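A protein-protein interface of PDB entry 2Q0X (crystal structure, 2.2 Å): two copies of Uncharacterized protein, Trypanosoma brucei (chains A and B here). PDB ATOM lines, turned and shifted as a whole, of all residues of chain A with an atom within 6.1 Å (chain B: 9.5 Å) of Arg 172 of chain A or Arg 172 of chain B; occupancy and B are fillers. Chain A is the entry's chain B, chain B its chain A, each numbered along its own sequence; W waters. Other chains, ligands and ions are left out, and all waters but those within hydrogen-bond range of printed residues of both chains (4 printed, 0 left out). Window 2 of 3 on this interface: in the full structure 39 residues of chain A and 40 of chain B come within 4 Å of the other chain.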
ATOM      1  N   PRO A  84       0.253  13.230 -11.186  1.00  0.00           N
ATOM      2  CA  PRO A  84      -0.453  12.093 -10.595  1.00  0.00           C
ATOM      3  C   PRO A  84      -0.034  10.742 -11.194  1.00  0.00           C
ATOM      4  O   PRO A  84       0.139  10.613 -12.407  1.00  0.00           O
ATOM      5  CB  PRO A  84      -1.915  12.391 -10.922  1.00  0.00           C
ATOM      6  CG  PRO A  84      -1.841  13.079 -12.235  1.00  0.00           C
ATOM      7  CD  PRO A  84      -0.591  13.927 -12.173  1.00  0.00           C
ATOM      8  N   LYS A 166      -8.619  12.871 -23.296  1.00  0.00           N
ATOM      9  CA  LYS A 166      -8.802  14.324 -23.388  1.00  0.00           C
ATOM     10  C   LYS A 166      -8.394  14.993 -22.092  1.00  0.00           C
ATOM     11  O   LYS A 166      -7.743  16.039 -22.104  1.00  0.00           O
ATOM     12  CB  LYS A 166     -10.259  14.674 -23.704  1.00  0.00           C
ATOM     13  N   LEU A 167      -8.790  14.389 -20.973  1.00  0.00           N
ATOM     14  CA  LEU A 167      -8.432  14.893 -19.654  1.00  0.00           C
ATOM     15  C   LEU A 167      -6.920  14.881 -19.464  1.00  0.00           C
ATOM     16  O   LEU A 167      -6.351  15.842 -18.942  1.00  0.00           O
ATOM     17  CB  LEU A 167      -9.114  14.076 -18.544  1.00  0.00           C
ATOM     18  CG  LEU A 167     -10.639  14.190 -18.439  1.00  0.00           C
ATOM     19  CD1 LEU A 167     -11.202  13.187 -17.449  1.00  0.00           C
ATOM     20  CD2 LEU A 167     -11.061  15.606 -18.062  1.00  0.00           C
ATOM     21  N   MET A 168      -6.272  13.797 -19.887  1.00  0.00           N
ATOM     22  CA  MET A 168      -4.816  13.727 -19.831  1.00  0.00           C
ATOM     23  C   MET A 168      -4.192  14.799 -20.728  1.00  0.00           C
ATOM     24  O   MET A 168      -3.184  15.410 -20.352  1.00  0.00           O
ATOM     25  CB  MET A 168      -4.307  12.337 -20.227  1.00  0.00           C
ATOM     26  CG  MET A 168      -4.720  11.210 -19.275  1.00  0.00           C
ATOM     27  SD  MET A 168      -4.360  11.479 -17.531  1.00  0.00           S
ATOM     28  CE  MET A 168      -2.570  11.326 -17.467  1.00  0.00           C
ATOM     29  N   ALA A 169      -4.817  15.046 -21.883  1.00  0.00           N
ATOM     30  CA  ALA A 169      -4.382  16.091 -22.821  1.00  0.00           C
ATOM     31  C   ALA A 169      -4.472  17.500 -22.225  1.00  0.00           C
ATOM     32  O   ALA A 169      -3.628  18.341 -22.510  1.00  0.00           O
ATOM     33  CB  ALA A 169      -5.186  16.013 -24.129  1.00  0.00           C
ATOM     34  N   GLU A 170      -5.489  17.743 -21.399  1.00  0.00           N
ATOM     35  CA  GLU A 170      -5.645  19.014 -20.670  1.00  0.00           C
ATOM     36  C   GLU A 170      -4.808  19.099 -19.382  1.00  0.00           C
ATOM     37  O   GLU A 170      -4.787  20.138 -18.733  1.00  0.00           O
ATOM     38  CB  GLU A 170      -7.125  19.250 -20.334  1.00  0.00           C
ATOM     39  CG  GLU A 170      -7.975  19.631 -21.550  1.00  0.00           C
ATOM     40  CD  GLU A 170      -9.378  19.019 -21.556  1.00  0.00           C
ATOM     41  OE1 GLU A 170      -9.723  18.254 -20.629  1.00  0.00           O
ATOM     42  OE2 GLU A 170     -10.137  19.296 -22.520  1.00  0.00           O
ATOM     43  N   GLY A 171      -4.121  18.019 -19.019  1.00  0.00           N
ATOM     44  CA  GLY A 171      -3.311  17.990 -17.807  1.00  0.00           C
ATOM     45  C   GLY A 171      -4.152  17.865 -16.544  1.00  0.00           C
ATOM     46  O   GLY A 171      -3.778  18.378 -15.476  1.00  0.00           O
ATOM     47  N   ARG A 172      -5.280  17.161 -16.667  1.00  0.00           N
ATOM     48  CA  ARG A 172      -6.249  17.022 -15.582  1.00  0.00           C
ATOM     49  C   ARG A 172      -6.311  15.586 -15.069  1.00  0.00           C
ATOM     50  O   ARG A 172      -7.378  15.089 -14.703  1.00  0.00           O
ATOM     51  CB  ARG A 172      -7.624  17.463 -16.066  1.00  0.00           C
ATOM     52  CG  ARG A 172      -7.651  18.873 -16.639  1.00  0.00           C
ATOM     53  CD  ARG A 172      -8.989  19.186 -17.248  1.00  0.00           C
ATOM     54  NE  ARG A 172     -10.101  19.054 -16.305  1.00  0.00           N
ATOM     55  CZ  ARG A 172     -11.383  19.221 -16.630  1.00  0.00           C
ATOM     56  NH1 ARG A 172     -11.725  19.515 -17.884  1.00  0.00           N
ATOM     57  NH2 ARG A 172     -12.334  19.086 -15.710  1.00  0.00           N
ATOM     58  N   GLY A 173      -5.152  14.937 -15.023  1.00  0.00           N
ATOM     59  CA  GLY A 173      -5.061  13.534 -14.642  1.00  0.00           C
ATOM     60  C   GLY A 173      -5.333  13.199 -13.184  1.00  0.00           C
ATOM     61  O   GLY A 173      -5.544  12.036 -12.849  1.00  0.00           O
ATOM     62  N   GLU A 174      -5.338  14.200 -12.311  1.00  0.00           N
ATOM     63  CA  GLU A 174      -5.565  13.960 -10.885  1.00  0.00           C
ATOM     64  C   GLU A 174      -7.009  14.235 -10.450  1.00  0.00           C
ATOM     65  O   GLU A 174      -7.382  13.933  -9.323  1.00  0.00           O
ATOM     66  CB  GLU A 174      -4.596  14.804 -10.063  1.00  0.00           C
ATOM     67  CG  GLU A 174      -4.447  14.353  -8.598  1.00  0.00           C
ATOM     68  CD  GLU A 174      -4.078  15.490  -7.679  1.00  0.00           C
ATOM     69  OE1 GLU A 174      -4.875  16.449  -7.595  1.00  0.00           O
ATOM     70  OE2 GLU A 174      -3.000  15.424  -7.040  1.00  0.00           O
ATOM     71  N   ASP A 175      -7.829  14.785 -11.337  1.00  0.00           N
ATOM     72  CA  ASP A 175      -9.183  15.180 -10.948  1.00  0.00           C
ATOM     73  C   ASP A 175     -10.169  14.023 -11.088  1.00  0.00           C
ATOM     74  O   ASP A 175     -10.746  13.809 -12.161  1.00  0.00           O
ATOM     75  CB  ASP A 175      -9.645  16.375 -11.780  1.00  0.00           C
ATOM     76  CG  ASP A 175     -11.028  16.891 -11.369  1.00  0.00           C
ATOM     77  OD1 ASP A 175     -11.449  16.669 -10.202  1.00  0.00           O
ATOM     78  OD2 ASP A 175     -11.683  17.531 -12.227  1.00  0.00           O
ATOM     79  N   SER A 176     -10.384  13.308  -9.988  1.00  0.00           N
ATOM     80  CA  SER A 176     -11.333  12.204  -9.969  1.00  0.00           C
ATOM     81  C   SER A 176     -12.766  12.637 -10.277  1.00  0.00           C
ATOM     82  O   SER A 176     -13.548  11.836 -10.800  1.00  0.00           O
ATOM     83  CB  SER A 176     -11.298  11.459  -8.631  1.00  0.00           C
ATOM     84  OG  SER A 176     -11.908  12.214  -7.603  1.00  0.00           O
ATOM     85  N   ALA A 178     -13.670  14.865 -12.504  1.00  0.00           N
ATOM     86  CA  ALA A 178     -13.801  14.958 -13.964  1.00  0.00           C
ATOM     87  C   ALA A 178     -14.212  13.613 -14.592  1.00  0.00           C
ATOM     88  O   ALA A 178     -14.570  13.558 -15.763  1.00  0.00           O
ATOM     89  CB  ALA A 178     -12.495  15.452 -14.579  1.00  0.00           C
ATOM     90  N   PRO A 189      -8.358  10.028 -13.662  1.00  0.00           N
ATOM     91  CA  PRO A 189      -8.101   9.788 -15.080  1.00  0.00           C
ATOM     92  C   PRO A 189      -6.712   9.179 -15.335  1.00  0.00           C
ATOM     93  O   PRO A 189      -6.568   8.349 -16.227  1.00  0.00           O
ATOM     94  CB  PRO A 189      -8.197  11.185 -15.700  1.00  0.00           C
ATOM     95  CG  PRO A 189      -9.086  11.936 -14.801  1.00  0.00           C
ATOM     96  CD  PRO A 189      -8.801  11.415 -13.413  1.00  0.00           C
ATOM     97  N   ALA A 190      -5.716   9.590 -14.553  1.00  0.00           N
ATOM     98  CA  ALA A 190      -4.348   9.080 -14.674  1.00  0.00           C
ATOM     99  C   ALA A 190      -4.213   7.566 -14.405  1.00  0.00           C
ATOM    100  O   ALA A 190      -3.383   6.887 -15.023  1.00  0.00           O
ATOM    101  CB  ALA A 190      -3.423   9.876 -13.749  1.00  0.00           C
ATOM    102  N   GLY B  83     -14.375  15.117  -1.445  1.00  0.00           N
ATOM    103  CA  GLY B  83     -15.472  16.074  -1.606  1.00  0.00           C
ATOM    104  C   GLY B  83     -15.465  16.777  -2.951  1.00  0.00           C
ATOM    105  O   GLY B  83     -16.353  16.552  -3.766  1.00  0.00           O
ATOM    106  N   PRO B  84     -14.453  17.631  -3.208  1.00  0.00           N
ATOM    107  CA  PRO B  84     -13.273  17.948  -2.404  1.00  0.00           C
ATOM    108  C   PRO B  84     -13.553  18.942  -1.270  1.00  0.00           C
ATOM    109  O   PRO B  84     -14.296  19.898  -1.443  1.00  0.00           O
ATOM    110  CB  PRO B  84     -12.316  18.556  -3.427  1.00  0.00           C
ATOM    111  CG  PRO B  84     -13.223  19.212  -4.421  1.00  0.00           C
ATOM    112  CD  PRO B  84     -14.478  18.396  -4.469  1.00  0.00           C
ATOM    113  N   HIS B 163      -8.260  32.906  -9.986  1.00  0.00           N
ATOM    114  CA  HIS B 163      -7.984  31.594 -10.588  1.00  0.00           C
ATOM    115  C   HIS B 163      -8.727  30.471  -9.865  1.00  0.00           C
ATOM    116  O   HIS B 163      -9.214  29.539 -10.509  1.00  0.00           O
ATOM    117  CB  HIS B 163      -6.472  31.320 -10.587  1.00  0.00           C
ATOM    118  CG  HIS B 163      -6.076  30.067 -11.311  1.00  0.00           C
ATOM    119  ND1 HIS B 163      -5.966  30.003 -12.683  1.00  0.00           N
ATOM    120  CD2 HIS B 163      -5.755  28.833 -10.851  1.00  0.00           C
ATOM    121  CE1 HIS B 163      -5.599  28.786 -13.039  1.00  0.00           C
ATOM    122  NE2 HIS B 163      -5.462  28.056 -11.947  1.00  0.00           N
ATOM    123  N   VAL B 164      -8.802  30.570  -8.536  1.00  0.00           N
ATOM    124  CA  VAL B 164      -9.511  29.599  -7.702  1.00  0.00           C
ATOM    125  C   VAL B 164     -11.030  29.658  -7.916  1.00  0.00           C
ATOM    126  O   VAL B 164     -11.688  28.623  -7.987  1.00  0.00           O
ATOM    127  CB  VAL B 164      -9.178  29.804  -6.189  1.00  0.00           C
ATOM    128  CG1 VAL B 164     -10.110  28.996  -5.299  1.00  0.00           C
ATOM    129  CG2 VAL B 164      -7.731  29.437  -5.908  1.00  0.00           C
ATOM    130  N   GLU B 165     -11.574  30.871  -7.998  1.00  0.00           N
ATOM    131  CA  GLU B 165     -12.998  31.089  -8.312  1.00  0.00           C
ATOM    132  C   GLU B 165     -13.408  30.429  -9.626  1.00  0.00           C
ATOM    133  O   GLU B 165     -14.497  29.850  -9.723  1.00  0.00           O
ATOM    134  CB  GLU B 165     -13.307  32.585  -8.404  1.00  0.00           C
ATOM    135  CG  GLU B 165     -13.313  33.298  -7.077  1.00  0.00           C
ATOM    136  CD  GLU B 165     -13.389  34.814  -7.219  1.00  0.00           C
ATOM    137  OE1 GLU B 165     -13.828  35.317  -8.284  1.00  0.00           O
ATOM    138  OE2 GLU B 165     -13.010  35.501  -6.247  1.00  0.00           O
ATOM    139  N   LYS B 166     -12.534  30.544 -10.626  1.00  0.00           N
ATOM    140  CA  LYS B 166     -12.770  29.989 -11.955  1.00  0.00           C
ATOM    141  C   LYS B 166     -12.794  28.465 -11.921  1.00  0.00           C
ATOM    142  O   LYS B 166     -13.680  27.853 -12.520  1.00  0.00           O
ATOM    143  CB  LYS B 166     -11.693  30.471 -12.932  1.00  0.00           C
ATOM    144  N   LEU B 167     -11.833  27.862 -11.214  1.00  0.00           N
ATOM    145  CA  LEU B 167     -11.754  26.399 -11.091  1.00  0.00           C
ATOM    146  C   LEU B 167     -12.943  25.832 -10.317  1.00  0.00           C
ATOM    147  O   LEU B 167     -13.480  24.790 -10.679  1.00  0.00           O
ATOM    148  CB  LEU B 167     -10.446  25.958 -10.427  1.00  0.00           C
ATOM    149  CG  LEU B 167      -9.122  26.193 -11.165  1.00  0.00           C
ATOM    150  CD1 LEU B 167      -7.943  25.869 -10.259  1.00  0.00           C
ATOM    151  CD2 LEU B 167      -9.023  25.386 -12.446  1.00  0.00           C
ATOM    152  N   MET B 168     -13.358  26.527  -9.264  1.00  0.00           N
ATOM    153  CA  MET B 168     -14.488  26.083  -8.438  1.00  0.00           C
ATOM    154  C   MET B 168     -15.794  26.090  -9.212  1.00  0.00           C
ATOM    155  O   MET B 168     -16.661  25.255  -8.952  1.00  0.00           O
ATOM    156  CB  MET B 168     -14.637  26.961  -7.186  1.00  0.00           C
ATOM    157  CG  MET B 168     -13.497  26.824  -6.175  1.00  0.00           C
ATOM    158  SD  MET B 168     -13.183  25.141  -5.632  1.00  0.00           S
ATOM    159  CE  MET B 168     -14.645  24.790  -4.657  1.00  0.00           C
ATOM    160  N   ALA B 169     -15.921  27.034 -10.146  1.00  0.00           N
ATOM    161  CA  ALA B 169     -17.092  27.144 -11.020  1.00  0.00           C
ATOM    162  C   ALA B 169     -17.114  26.042 -12.080  1.00  0.00           C
ATOM    163  O   ALA B 169     -18.180  25.634 -12.531  1.00  0.00           O
ATOM    164  CB  ALA B 169     -17.127  28.508 -11.686  1.00  0.00           C
ATOM    165  N   GLU B 170     -15.934  25.576 -12.477  1.00  0.00           N
ATOM    166  CA  GLU B 170     -15.816  24.433 -13.388  1.00  0.00           C
ATOM    167  C   GLU B 170     -15.992  23.084 -12.686  1.00  0.00           C
ATOM    168  O   GLU B 170     -16.132  22.056 -13.348  1.00  0.00           O
ATOM    169  CB  GLU B 170     -14.474  24.490 -14.124  1.00  0.00           C
ATOM    170  CG  GLU B 170     -14.346  25.745 -14.998  1.00  0.00           C
ATOM    171  CD  GLU B 170     -12.964  25.922 -15.601  1.00  0.00           C
ATOM    172  OE1 GLU B 170     -11.972  25.629 -14.905  1.00  0.00           O
ATOM    173  OE2 GLU B 170     -12.875  26.363 -16.770  1.00  0.00           O
ATOM    174  N   GLY B 171     -15.996  23.085 -11.355  1.00  0.00           N
ATOM    175  CA  GLY B 171     -16.071  21.845 -10.585  1.00  0.00           C
ATOM    176  C   GLY B 171     -14.712  21.179 -10.456  1.00  0.00           C
ATOM    177  O   GLY B 171     -14.628  19.965 -10.300  1.00  0.00           O
ATOM    178  N   ARG B 172     -13.652  21.984 -10.515  1.00  0.00           N
ATOM    179  CA  ARG B 172     -12.278  21.495 -10.531  1.00  0.00           C
ATOM    180  C   ARG B 172     -11.594  21.691  -9.177  1.00  0.00           C
ATOM    181  O   ARG B 172     -10.359  21.731  -9.097  1.00  0.00           O
ATOM    182  CB  ARG B 172     -11.472  22.209 -11.618  1.00  0.00           C
ATOM    183  CG  ARG B 172     -11.882  21.886 -13.052  1.00  0.00           C
ATOM    184  CD  ARG B 172     -10.651  21.597 -13.898  1.00  0.00           C
ATOM    185  NE  ARG B 172     -10.202  22.730 -14.694  1.00  0.00           N
ATOM    186  CZ  ARG B 172      -8.946  22.933 -15.106  1.00  0.00           C
ATOM    187  NH1 ARG B 172      -7.959  22.095 -14.793  1.00  0.00           N
ATOM    188  NH2 ARG B 172      -8.674  24.009 -15.840  1.00  0.00           N
ATOM    189  N   GLY B 173     -12.399  21.777  -8.114  1.00  0.00           N
ATOM    190  CA  GLY B 173     -11.899  21.976  -6.749  1.00  0.00           C
ATOM    191  C   GLY B 173     -10.860  20.986  -6.235  1.00  0.00           C
ATOM    192  O   GLY B 173     -10.056  21.338  -5.372  1.00  0.00           O
ATOM    193  N   GLU B 174     -10.870  19.754  -6.762  1.00  0.00           N
ATOM    194  CA  GLU B 174      -9.913  18.704  -6.367  1.00  0.00           C
ATOM    195  C   GLU B 174      -8.604  18.741  -7.168  1.00  0.00           C
ATOM    196  O   GLU B 174      -7.699  17.968  -6.904  1.00  0.00           O
ATOM    197  CB  GLU B 174     -10.551  17.313  -6.522  1.00  0.00           C
ATOM    198  CG  GLU B 174      -9.841  16.178  -5.737  1.00  0.00           C
ATOM    199  CD  GLU B 174     -10.394  14.773  -6.036  1.00  0.00           C
ATOM    200  OE1 GLU B 174     -10.397  14.343  -7.216  1.00  0.00           O
ATOM    201  OE2 GLU B 174     -10.812  14.091  -5.078  1.00  0.00           O
ATOM    202  N   ASP B 175      -8.492  19.634  -8.143  1.00  0.00           N
ATOM    203  CA  ASP B 175      -7.373  19.566  -9.079  1.00  0.00           C
ATOM    204  C   ASP B 175      -6.188  20.416  -8.610  1.00  0.00           C
ATOM    205  O   ASP B 175      -6.048  21.577  -8.999  1.00  0.00           O
ATOM    206  CB  ASP B 175      -7.847  19.985 -10.471  1.00  0.00           C
ATOM    207  CG  ASP B 175      -6.861  19.621 -11.565  1.00  0.00           C
ATOM    208  OD1 ASP B 175      -5.800  19.042 -11.251  1.00  0.00           O
ATOM    209  OD2 ASP B 175      -7.155  19.928 -12.743  1.00  0.00           O
ATOM    210  N   SER B 176      -5.325  19.826  -7.789  1.00  0.00           N
ATOM    211  CA  SER B 176      -4.187  20.556  -7.237  1.00  0.00           C
ATOM    212  C   SER B 176      -3.176  20.965  -8.313  1.00  0.00           C
ATOM    213  O   SER B 176      -2.483  21.970  -8.166  1.00  0.00           O
ATOM    214  CB  SER B 176      -3.500  19.743  -6.126  1.00  0.00           C
ATOM    215  OG  SER B 176      -2.683  18.703  -6.636  1.00  0.00           O
ATOM    216  N   LEU B 177      -3.102  20.182  -9.391  1.00  0.00           N
ATOM    217  CA  LEU B 177      -2.198  20.476 -10.511  1.00  0.00           C
ATOM    218  C   LEU B 177      -2.572  21.762 -11.251  1.00  0.00           C
ATOM    219  O   LEU B 177      -1.705  22.403 -11.855  1.00  0.00           O
ATOM    220  CB  LEU B 177      -2.100  19.293 -11.501  1.00  0.00           C
ATOM    221  CG  LEU B 177      -0.890  18.365 -11.300  1.00  0.00           C
ATOM    222  CD1 LEU B 177      -0.991  17.565 -10.021  1.00  0.00           C
ATOM    223  CD2 LEU B 177      -0.723  17.425 -12.482  1.00  0.00           C
ATOM    224  N   ALA B 178      -3.853  22.133 -11.196  1.00  0.00           N
ATOM    225  CA  ALA B 178      -4.321  23.412 -11.743  1.00  0.00           C
ATOM    226  C   ALA B 178      -3.805  24.629 -10.949  1.00  0.00           C
ATOM    227  O   ALA B 178      -3.885  25.752 -11.432  1.00  0.00           O
ATOM    228  CB  ALA B 178      -5.855  23.435 -11.812  1.00  0.00           C
ATOM    229  N   MET B 179      -3.280  24.396  -9.747  1.00  0.00           N
ATOM    230  CA  MET B 179      -2.768  25.467  -8.873  1.00  0.00           C
ATOM    231  C   MET B 179      -1.259  25.718  -8.968  1.00  0.00           C
ATOM    232  O   MET B 179      -0.718  26.499  -8.175  1.00  0.00           O
ATOM    233  CB  MET B 179      -3.092  25.146  -7.401  1.00  0.00           C
ATOM    234  CG  MET B 179      -4.532  25.275  -7.026  1.00  0.00           C
ATOM    235  SD  MET B 179      -5.170  26.898  -7.393  1.00  0.00           S
ATOM    236  CE  MET B 179      -3.858  28.003  -6.838  1.00  0.00           C
ATOM    237  N   LEU B 180      -0.573  25.091  -9.916  1.00  0.00           N
ATOM    238  CA  LEU B 180       0.895  25.061  -9.858  1.00  0.00           C
ATOM    239  C   LEU B 180       1.578  26.400 -10.175  1.00  0.00           C
ATOM    240  O   LEU B 180       2.659  26.670  -9.656  1.00  0.00           O
ATOM    241  CB  LEU B 180       1.480  23.932 -10.730  1.00  0.00           C
ATOM    242  CG  LEU B 180       1.846  22.624  -9.992  1.00  0.00           C
ATOM    243  CD1 LEU B 180       0.711  21.642 -10.038  1.00  0.00           C
ATOM    244  CD2 LEU B 180       3.099  21.974 -10.584  1.00  0.00           C
ATOM    245  N   LYS B 181       0.960  27.244 -10.995  1.00  0.00           N
ATOM    246  CA  LYS B 181       1.588  28.521 -11.347  1.00  0.00           C
ATOM    247  C   LYS B 181       1.140  29.633 -10.392  1.00  0.00           C
ATOM    248  O   LYS B 181       1.823  30.639 -10.237  1.00  0.00           O
ATOM    249  CB  LYS B 181       1.350  28.866 -12.839  1.00  0.00           C
ATOM    250  CG  LYS B 181       0.276  29.912 -13.132  1.00  0.00           C
ATOM    251  CD  LYS B 181       0.100  30.149 -14.630  1.00  0.00           C
ATOM    252  CE  LYS B 181      -0.690  29.034 -15.331  1.00  0.00           C
ATOM    253  NZ  LYS B 181       0.170  28.085 -16.115  1.00  0.00           N
ATOM    254  N   ILE B 187      -1.573  22.153  -3.117  1.00  0.00           N
ATOM    255  CA  ILE B 187      -2.838  22.539  -2.500  1.00  0.00           C
ATOM    256  C   ILE B 187      -3.974  22.453  -3.520  1.00  0.00           C
ATOM    257  O   ILE B 187      -3.780  22.763  -4.711  1.00  0.00           O
ATOM    258  CB  ILE B 187      -2.746  23.977  -1.906  1.00  0.00           C
ATOM    259  CG1 ILE B 187      -4.004  24.331  -1.100  1.00  0.00           C
ATOM    260  CG2 ILE B 187      -2.495  25.016  -3.016  1.00  0.00           C
ATOM    261  CD1 ILE B 187      -3.798  25.466  -0.100  1.00  0.00           C
ATOM    262  N   THR B 188      -5.151  22.019  -3.070  1.00  0.00           N
ATOM    263  CA  THR B 188      -6.301  21.937  -3.958  1.00  0.00           C
ATOM    264  C   THR B 188      -6.987  23.298  -4.027  1.00  0.00           C
ATOM    265  O   THR B 188      -6.953  24.052  -3.058  1.00  0.00           O
ATOM    266  CB  THR B 188      -7.314  20.834  -3.539  1.00  0.00           C
ATOM    267  OG1 THR B 188      -7.809  21.085  -2.220  1.00  0.00           O
ATOM    268  CG2 THR B 188      -6.683  19.468  -3.596  1.00  0.00           C
ATOM    269  N   PRO B 189      -7.572  23.641  -5.190  1.00  0.00           N
ATOM    270  CA  PRO B 189      -8.381  24.866  -5.250  1.00  0.00           C
ATOM    271  C   PRO B 189      -9.447  24.940  -4.145  1.00  0.00           C
ATOM    272  O   PRO B 189      -9.653  26.009  -3.569  1.00  0.00           O
ATOM    273  CB  PRO B 189      -9.015  24.813  -6.644  1.00  0.00           C
ATOM    274  CG  PRO B 189      -8.069  23.975  -7.465  1.00  0.00           C
ATOM    275  CD  PRO B 189      -7.478  22.967  -6.497  1.00  0.00           C
ATOM    276  N   ALA B 190     -10.083  23.811  -3.840  1.00  0.00           N
ATOM    277  CA  ALA B 190     -11.113  23.759  -2.810  1.00  0.00           C
ATOM    278  C   ALA B 190     -10.584  24.177  -1.447  1.00  0.00           C
ATOM    279  O   ALA B 190     -11.310  24.762  -0.669  1.00  0.00           O
ATOM    280  CB  ALA B 190     -11.731  22.377  -2.731  1.00  0.00           C
ATOM    281  N   ARG B 191      -9.329  23.869  -1.143  1.00  0.00           N
ATOM    282  CA  ARG B 191      -8.737  24.314   0.121  1.00  0.00           C
ATOM    283  C   ARG B 191      -8.470  25.830   0.134  1.00  0.00           C
ATOM    284  O   ARG B 191      -8.637  26.479   1.154  1.00  0.00           O
ATOM    285  CB  ARG B 191      -7.475  23.503   0.461  1.00  0.00           C
ATOM    286  CG  ARG B 191      -7.792  22.145   1.088  1.00  0.00           C
ATOM    287  CD  ARG B 191      -8.291  22.278   2.541  1.00  0.00           C
ATOM    288  NE  ARG B 191      -7.308  22.927   3.422  1.00  0.00           N
ATOM    289  CZ  ARG B 191      -6.287  22.312   4.020  1.00  0.00           C
ATOM    290  NH1 ARG B 191      -6.076  21.007   3.866  1.00  0.00           N
ATOM    291  NH2 ARG B 191      -5.449  23.006   4.778  1.00  0.00           N
ATOM    292  N   ALA B 193     -10.266  28.018  -1.677  1.00  0.00           N
ATOM    293  CA  ALA B 193     -11.538  28.723  -1.933  1.00  0.00           C
ATOM    294  C   ALA B 193     -12.346  29.105  -0.685  1.00  0.00           C
ATOM    295  O   ALA B 193     -13.069  30.099  -0.688  1.00  0.00           O
ATOM    296  CB  ALA B 193     -12.416  27.911  -2.903  1.00  0.00           C
HETATM  297  O   HOH W   1     -12.528  18.602  -8.820  1.00  0.00           O
HETATM  298  O   HOH W   2      -9.842  19.011 -12.917  1.00  0.00           O
HETATM  299  O   HOH W   3      -4.745  17.205 -12.515  1.00  0.00           O
HETATM  300  O   HOH W   4      -5.166  20.767 -14.156  1.00  0.00           O
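Among the printed residues, pairs that only touch across the chains: Pro 84 of chain A with Leu 177 of chain B (3.5 Å), Arg 172 of chain A with Arg 172 of chain B (3.5 Å) and Asp 175 of chain A with Glu 174 of chain B (3.8 Å).
Of chain B, only Arg 172 comes within 4 Å of Arg 172 of chain A. Of chain A, only Arg 172 comes within 4 Å of Arg 172 of chain B. No residue of chain B comes within 4 Å of Glu 170 of chain A. No residue of chain B comes within 4 Å of Gly 171 of chain A. No residue of chain B comes within 4 Å of Gly 173 of chain A. Of the printed residues of chain B, Asp 175 of chain A touches Glu 174 (3.8 Å). Of the printed residues of chain B, Ser 176 of chain A touches Glu 174. Printed residues of chain A within 4 Å of Leu 177 of chain B: Pro 84 (3.5 Å). Of the printed residues of chain B, Glu 174 of chain A touches Glu 174 and Ser 176. Of the printed residues of chain A, Glu 174 of chain B touches Glu 174 (3.3 Å), Asp 175 (3.8 Å) and Ser 176 (2.6 Å). Printed residues of chain A within 4 Å of Ser 176 of chain B: Glu 174 (3.3 Å). Leu 167 of chain A touches none of the printed residues of chain B. Glu 165 of chain B touches none of the printed residues of chain A. The nearest residue of chain A that does not touch Arg 172 of chain B is Asp 175 of chain A (4.4 Å). The nearest printed residue of chain B that does not touch Pro 84 of chain A is Asp 175 of chain B (7.2 Å).
Water W2 lies within hydrogen-bond range of the side-chain carboxylate (OD2) of Asp 175 of chain A, the side-chain carboxylate (OD2) of Asp 175 of chain B and the guanidinium group (NE) of Arg 172 of chain A. Water W4 lies within hydrogen-bond range of the side-chain carboxylate of Asp 175 of chain B (2.6 Å), the backbone carbonyl oxygen of Gly 171 of chain A (3.1 Å) and the guanidinium group of Arg 172 of chain B (3.2 Å). Water W1 lies within hydrogen-bond range of the side-chain carboxylate of Asp 175 of chain A, the backbone NH of Glu 174 of chain B, the backbone carbonyl oxygen of Gly 171 of chain B and the backbone NH of Gly 173 of chain B.
Arg 172 of chain B touches its own counterpart, Arg 172 of chain A. Glu 174 of chain A touches its own counterpart, Glu 174 of chain B. Glu 174 of chain A touches Ser 176 of chain B, and with the chains exchanged Ser 176 of chain A touches Glu 174 of chain B. Asp 175 of chain A touches Glu 174 of chain B, but with the chains exchanged Glu 174 of chain A does not touch Asp 175 of chain B (4.3 Å).
N of Arg 172 of chain B sits at hydrogen-bond distance from O of Leu 167 of chain B (2.8 Å). The side-chain carboxylate of Glu 170 of chain B is in salt-bridge range of the guanidinium group of Arg 172 of chain B (3.4 Å). The side-chain carboxylate (OD2) of Asp 175 of chain B lies within salt-bridge range of the guanidinium group (NH1) of Arg 172 of chain B (3.1 Å). N of Arg 172 of chain A lies within hydrogen-bond range of O of Leu 167 of chain A, 2.8 Å away. OE1 of Glu 170 of chain A lies within salt-bridge range of NH1 of Arg 172 of chain A, 3.6 Å away. The side-chain carboxylate (OD2) of Asp 175 of chain A sits close to the backbone NH (N) of Ala 178 of chain A, at 3.3 Å.
Of the 15 printed residues of chain A, 5 touch a printed residue of chain B. Hydrophobic or aromatic side chains of chain B that line the printed part of chain A: Leu 177. Among the printed residues, 6 pairs touch across the chains.
OG of Ser 176 of chain A sits at hydrogen-bond distance from OE1 of Glu 174 of chain B. OE1 of Glu 174 of chain A is in hydrogen-bond range of OG of Ser 176 of chain B (3.3 Å). The side-chain carboxylate of Glu 174 of chain A lies close to the backbone carbonyl oxygen of Glu 174 of chain B (3.3 Å).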
